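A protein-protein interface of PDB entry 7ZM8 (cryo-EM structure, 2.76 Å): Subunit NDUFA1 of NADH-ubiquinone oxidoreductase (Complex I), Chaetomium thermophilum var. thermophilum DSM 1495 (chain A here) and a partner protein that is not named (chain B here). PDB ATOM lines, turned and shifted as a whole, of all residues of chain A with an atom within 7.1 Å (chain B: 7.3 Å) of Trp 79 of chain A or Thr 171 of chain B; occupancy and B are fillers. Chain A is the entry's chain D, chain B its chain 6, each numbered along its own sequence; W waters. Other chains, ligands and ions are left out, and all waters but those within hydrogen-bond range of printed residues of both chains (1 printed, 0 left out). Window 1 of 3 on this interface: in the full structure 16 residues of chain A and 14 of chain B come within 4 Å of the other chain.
The backbone NH (N) of Thr 171 of chain B lies within hydrogen-bond range of the backbone carbonyl oxygen (O) of Lys 80 of chain A, at 2.9 Å.
The side-chain amino group of Lys 80 of chain A is in salt-bridge range of the side-chain carboxylate of Glu 12 of chain B, 3.4 Å away.
O of UNK 82 of chain A sits at hydrogen-bond distance from N of Phe 169 of chain B (2.8 Å).
Trp 79 of chain A touches Ile 170 of chain B.
Trp 79 of chain A touches Thr 171 of chain B (CA to O, 3.4 Å).
Trp 79 of chain A touches Ser 172 of chain B.
Lys 80 of chain A touches Phe 169 of chain B.
O of Lys 80 of chain A touches CA of Ile 170 of chain B, at 3.6 Å.
Phe 168 of chain B touches Val 81 of chain A.
Phe 169 of chain B touches Val 81 of chain A (O to CA, 3.6 Å).
O of UNK 82 of chain A touches CD2 of Phe 168 of chain B, 3.2 Å away.
O of UNK 85 of chain A touches CG of Phe 169 of chain B (3.5 Å).
Trp 79 of chain A touches just these residues of chain B: Ile 170, Thr 171 and Ser 172.
Of chain A, only Trp 79 and Lys 80 come within 4 Å of Thr 171 of chain B.
Printed residues of chain B within 4 Å of UNK 82 of chain A: Phe 168 (3.2 Å) and Phe 169 (2.8 Å).
Printed residues of chain A within 4 Å of Ser 172 of chain B: Trp 79 (3.5 Å).
Printed residues of chain A within 4 Å of Phe 169 of chain B: Lys 80, Val 81, UNK 82 and UNK 85.
Of the printed residues of chain B, UNK 85 of chain A touches Phe 169 (3.5 Å).
Printed residues of chain B within 4 Å of Lys 80 of chain A: Glu 12 (3.3 Å), Phe 169 (3.8 Å), Ile 170 (3.6 Å) and Thr 171 (2.9 Å).
Printed residues of chain A that touch a printed residue of chain B: Trp 79, Lys 80, Val 81, UNK 82 and UNK 85.
Hydrophobic or aromatic side chains of chain A within 4 Å of the printed part of chain B: Trp 79 and Val 81.
Of the 8 printed residues of chain B, 6 touch a printed residue of chain A.
Hydrophobic or aromatic side chains of chain B within 4 Å of the printed part of chain A: Phe 168, Phe 169 and Ile 170.
Among the printed residues, 12 pairs touch across the chains.
Water W1 lies within hydrogen-bond range of the side-chain hydroxyl of Thr 171 of chain B (2.7 Å), the backbone carbonyl oxygen of Phe 169 of chain B (2.9 Å), the backbone carbonyl oxygen of Lys 80 of chain A (3.2 Å) and N of UNK 82 of chain A (3.5 Å).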
ATOM      1  N   ASN A  76     -17.613 -11.493  -1.902  1.00  0.00           N
ATOM      2  CA  ASN A  76     -17.395 -10.338  -0.987  1.00  0.00           C
ATOM      3  C   ASN A  76     -15.910 -10.079  -0.704  1.00  0.00           C
ATOM      4  O   ASN A  76     -15.631  -9.305   0.221  1.00  0.00           O
ATOM      5  CB  ASN A  76     -18.181 -10.504   0.316  1.00  0.00           C
ATOM      6  CG  ASN A  76     -17.867 -11.770   1.084  1.00  0.00           C
ATOM      7  OD1 ASN A  76     -16.843 -12.407   0.864  1.00  0.00           O
ATOM      8  ND2 ASN A  76     -18.740 -12.135   2.005  1.00  0.00           N
ATOM      9  N   ASN A  77     -15.004 -10.680  -1.472  1.00  0.00           N
ATOM     10  CA  ASN A  77     -13.582 -10.454  -1.263  1.00  0.00           C
ATOM     11  C   ASN A  77     -13.240  -9.020  -1.642  1.00  0.00           C
ATOM     12  O   ASN A  77     -13.434  -8.634  -2.801  1.00  0.00           O
ATOM     13  CB  ASN A  77     -12.776 -11.441  -2.094  1.00  0.00           C
ATOM     14  CG  ASN A  77     -11.333 -11.522  -1.665  1.00  0.00           C
ATOM     15  OD1 ASN A  77     -10.988 -11.202  -0.533  1.00  0.00           O
ATOM     16  ND2 ASN A  77     -10.473 -11.955  -2.577  1.00  0.00           N
ATOM     17  N   PRO A  78     -12.777  -8.157  -0.706  1.00  0.00           N
ATOM     18  CA  PRO A  78     -12.618  -6.748  -1.019  1.00  0.00           C
ATOM     19  C   PRO A  78     -11.360  -6.447  -1.822  1.00  0.00           C
ATOM     20  O   PRO A  78     -10.293  -6.832  -1.412  1.00  0.00           O
ATOM     21  CB  PRO A  78     -12.564  -6.049   0.345  1.00  0.00           C
ATOM     22  CG  PRO A  78     -12.739  -7.141   1.377  1.00  0.00           C
ATOM     23  CD  PRO A  78     -12.337  -8.416   0.678  1.00  0.00           C
ATOM     24  N   TRP A  79     -11.506  -5.763  -2.955  1.00  0.00           N
ATOM     25  CA  TRP A  79     -10.285  -5.255  -3.625  1.00  0.00           C
ATOM     26  C   TRP A  79     -10.231  -3.746  -3.425  1.00  0.00           C
ATOM     27  O   TRP A  79     -11.045  -3.048  -4.037  1.00  0.00           O
ATOM     28  CB  TRP A  79     -10.260  -5.657  -5.105  1.00  0.00           C
ATOM     29  CG  TRP A  79      -9.904  -7.086  -5.377  1.00  0.00           C
ATOM     30  CD1 TRP A  79      -9.924  -8.126  -4.495  1.00  0.00           C
ATOM     31  CD2 TRP A  79      -9.479  -7.640  -6.636  1.00  0.00           C
ATOM     32  NE1 TRP A  79      -9.539  -9.283  -5.112  1.00  0.00           N
ATOM     33  CE2 TRP A  79      -9.259  -9.017  -6.426  1.00  0.00           C
ATOM     34  CE3 TRP A  79      -9.267  -7.114  -7.914  1.00  0.00           C
ATOM     35  CZ2 TRP A  79      -8.832  -9.867  -7.444  1.00  0.00           C
ATOM     36  CZ3 TRP A  79      -8.848  -7.953  -8.920  1.00  0.00           C
ATOM     37  CH2 TRP A  79      -8.632  -9.311  -8.685  1.00  0.00           C
ATOM     38  N   LYS A  80      -9.328  -3.276  -2.575  1.00  0.00           N
ATOM     39  CA  LYS A  80      -9.243  -1.833  -2.256  1.00  0.00           C
ATOM     40  C   LYS A  80      -8.921  -1.037  -3.520  1.00  0.00           C
ATOM     41  O   LYS A  80      -8.075  -1.480  -4.302  1.00  0.00           O
ATOM     42  CB  LYS A  80      -8.171  -1.603  -1.188  1.00  0.00           C
ATOM     43  CG  LYS A  80      -8.267  -2.478   0.053  1.00  0.00           C
ATOM     44  CD  LYS A  80      -9.658  -2.569   0.631  1.00  0.00           C
ATOM     45  CE  LYS A  80      -9.701  -3.227   1.992  1.00  0.00           C
ATOM     46  NZ  LYS A  80      -8.998  -2.416   3.013  1.00  0.00           N
ATOM     47  N   VAL A  81      -9.664   0.128  -3.664  1.00  0.00           N
ATOM     48  CA  VAL A  81      -9.427   1.036  -4.824  1.00  0.00           C
ATOM     49  C   VAL A  81      -8.857   2.360  -4.304  1.00  0.00           C
ATOM     50  O   VAL A  81      -9.381   2.864  -3.296  1.00  0.00           O
ATOM     51  CB  VAL A  81     -10.681   1.221  -5.702  1.00  0.00           C
ATOM     52  CG1 VAL A  81     -10.322   1.187  -7.175  1.00  0.00           C
ATOM     53  CG2 VAL A  81     -11.748   0.183  -5.411  1.00  0.00           C
ATOM     54  N   UNK A  82      -7.759   2.866  -4.980  1.00  0.00           N
ATOM     55  CA  UNK A  82      -7.134   4.134  -4.539  1.00  0.00           C
ATOM     56  C   UNK A  82      -7.127   5.085  -5.728  1.00  0.00           C
ATOM     57  O   UNK A  82      -7.382   4.627  -6.843  1.00  0.00           O
ATOM     58  CB  UNK A  82      -5.737   3.900  -4.017  1.00  0.00           C
ATOM     59  N   UNK A  85      -1.967   6.769  -4.536  1.00  0.00           N
ATOM     60  CA  UNK A  85      -0.820   5.902  -4.164  1.00  0.00           C
ATOM     61  C   UNK A  85      -0.580   4.777  -5.167  1.00  0.00           C
ATOM     62  O   UNK A  85      -1.545   4.302  -5.781  1.00  0.00           O
ATOM     63  CB  UNK A  85      -0.980   5.340  -2.789  1.00  0.00           C
ATOM     64  N   LEU B   9     -19.253  -0.459  -6.425  1.00  0.00           N
ATOM     65  CA  LEU B   9     -18.297   0.425  -5.703  1.00  0.00           C
ATOM     66  C   LEU B   9     -18.875   0.801  -4.332  1.00  0.00           C
ATOM     67  O   LEU B   9     -20.018   1.270  -4.300  1.00  0.00           O
ATOM     68  CB  LEU B   9     -18.028   1.658  -6.569  1.00  0.00           C
ATOM     69  CG  LEU B   9     -16.698   2.366  -6.321  1.00  0.00           C
ATOM     70  CD1 LEU B   9     -15.537   1.390  -6.425  1.00  0.00           C
ATOM     71  CD2 LEU B   9     -16.516   3.512  -7.301  1.00  0.00           C
ATOM     72  N   GLU B  12     -15.170   1.972   2.120  1.00  0.00           N
ATOM     73  CA  GLU B  12     -14.628   1.161   3.242  1.00  0.00           C
ATOM     74  C   GLU B  12     -14.974   1.820   4.580  1.00  0.00           C
ATOM     75  O   GLU B  12     -15.082   3.056   4.611  1.00  0.00           O
ATOM     76  CB  GLU B  12     -13.122   0.995   3.081  1.00  0.00           C
ATOM     77  CG  GLU B  12     -12.710   0.695   1.658  1.00  0.00           C
ATOM     78  CD  GLU B  12     -11.210   0.611   1.470  1.00  0.00           C
ATOM     79  OE1 GLU B  12     -10.759   0.540   0.315  1.00  0.00           O
ATOM     80  OE2 GLU B  12     -10.500   0.613   2.484  1.00  0.00           O
ATOM     81  N   PHE B 168      -8.252   4.250 -11.519  1.00  0.00           N
ATOM     82  CA  PHE B 168      -8.138   4.011 -10.063  1.00  0.00           C
ATOM     83  C   PHE B 168      -7.111   2.892  -9.914  1.00  0.00           C
ATOM     84  O   PHE B 168      -7.053   2.042 -10.797  1.00  0.00           O
ATOM     85  CB  PHE B 168      -9.492   3.623  -9.467  1.00  0.00           C
ATOM     86  CG  PHE B 168     -10.383   4.773  -9.073  1.00  0.00           C
ATOM     87  CD1 PHE B 168     -11.188   5.403 -10.007  1.00  0.00           C
ATOM     88  CD2 PHE B 168     -10.432   5.212  -7.761  1.00  0.00           C
ATOM     89  CE1 PHE B 168     -12.012   6.455  -9.641  1.00  0.00           C
ATOM     90  CE2 PHE B 168     -11.256   6.265  -7.395  1.00  0.00           C
ATOM     91  CZ  PHE B 168     -12.044   6.884  -8.336  1.00  0.00           C
ATOM     92  N   PHE B 169      -6.358   2.885  -8.815  1.00  0.00           N
ATOM     93  CA  PHE B 169      -5.331   1.841  -8.575  1.00  0.00           C
ATOM     94  C   PHE B 169      -5.959   0.728  -7.740  1.00  0.00           C
ATOM     95  O   PHE B 169      -6.343   0.985  -6.599  1.00  0.00           O
ATOM     96  CB  PHE B 169      -4.134   2.437  -7.836  1.00  0.00           C
ATOM     97  CG  PHE B 169      -3.184   3.225  -8.695  1.00  0.00           C
ATOM     98  CD1 PHE B 169      -2.147   2.594  -9.360  1.00  0.00           C
ATOM     99  CD2 PHE B 169      -3.322   4.596  -8.830  1.00  0.00           C
ATOM    100  CE1 PHE B 169      -1.269   3.319 -10.147  1.00  0.00           C
ATOM    101  CE2 PHE B 169      -2.444   5.319  -9.617  1.00  0.00           C
ATOM    102  CZ  PHE B 169      -1.420   4.678 -10.273  1.00  0.00           C
ATOM    103  N   ILE B 170      -6.055  -0.469  -8.308  1.00  0.00           N
ATOM    104  CA  ILE B 170      -6.678  -1.623  -7.597  1.00  0.00           C
ATOM    105  C   ILE B 170      -5.612  -2.405  -6.825  1.00  0.00           C
ATOM    106  O   ILE B 170      -4.490  -2.521  -7.324  1.00  0.00           O
ATOM    107  CB  ILE B 170      -7.510  -2.509  -8.554  1.00  0.00           C
ATOM    108  CG1 ILE B 170      -8.452  -3.453  -7.803  1.00  0.00           C
ATOM    109  CG2 ILE B 170      -6.639  -3.248  -9.555  1.00  0.00           C
ATOM    110  CD1 ILE B 170      -9.768  -2.825  -7.431  1.00  0.00           C
ATOM    111  N   THR B 171      -5.947  -2.861  -5.620  1.00  0.00           N
ATOM    112  CA  THR B 171      -5.017  -3.714  -4.845  1.00  0.00           C
ATOM    113  C   THR B 171      -5.775  -4.889  -4.234  1.00  0.00           C
ATOM    114  O   THR B 171      -6.941  -4.708  -3.884  1.00  0.00           O
ATOM    115  CB  THR B 171      -4.303  -2.939  -3.727  1.00  0.00           C
ATOM    116  OG1 THR B 171      -5.251  -2.142  -3.018  1.00  0.00           O
ATOM    117  CG2 THR B 171      -3.163  -2.077  -4.218  1.00  0.00           C
ATOM    118  N   SER B 172      -5.129  -6.045  -4.106  1.00  0.00           N
ATOM    119  CA  SER B 172      -5.726  -7.200  -3.451  1.00  0.00           C
ATOM    120  C   SER B 172      -4.738  -7.776  -2.450  1.00  0.00           C
ATOM    121  O   SER B 172      -3.654  -7.219  -2.256  1.00  0.00           O
ATOM    122  CB  SER B 172      -6.133  -8.253  -4.479  1.00  0.00           C
ATOM    123  OG  SER B 172      -6.272  -9.524  -3.875  1.00  0.00           O
ATOM    124  N   LYS B 173      -5.105  -8.881  -1.788  1.00  0.00           N
ATOM    125  CA  LYS B 173      -4.284  -9.487  -0.708  1.00  0.00           C
ATOM    126  C   LYS B 173      -3.502 -10.710  -1.198  1.00  0.00           C
ATOM    127  O   LYS B 173      -3.959 -11.338  -2.155  1.00  0.00           O
ATOM    128  CB  LYS B 173      -5.248  -9.842   0.428  1.00  0.00           C
ATOM    129  CG  LYS B 173      -6.089 -11.095   0.260  1.00  0.00           C
ATOM    130  CD  LYS B 173      -6.830 -11.463   1.526  1.00  0.00           C
ATOM    131  CE  LYS B 173      -7.409 -10.265   2.249  1.00  0.00           C
ATOM    132  NZ  LYS B 173      -8.414 -10.652   3.269  1.00  0.00           N
HETATM  133  O   HOH W   1      -5.503   0.413  -3.914  1.00  0.00           O
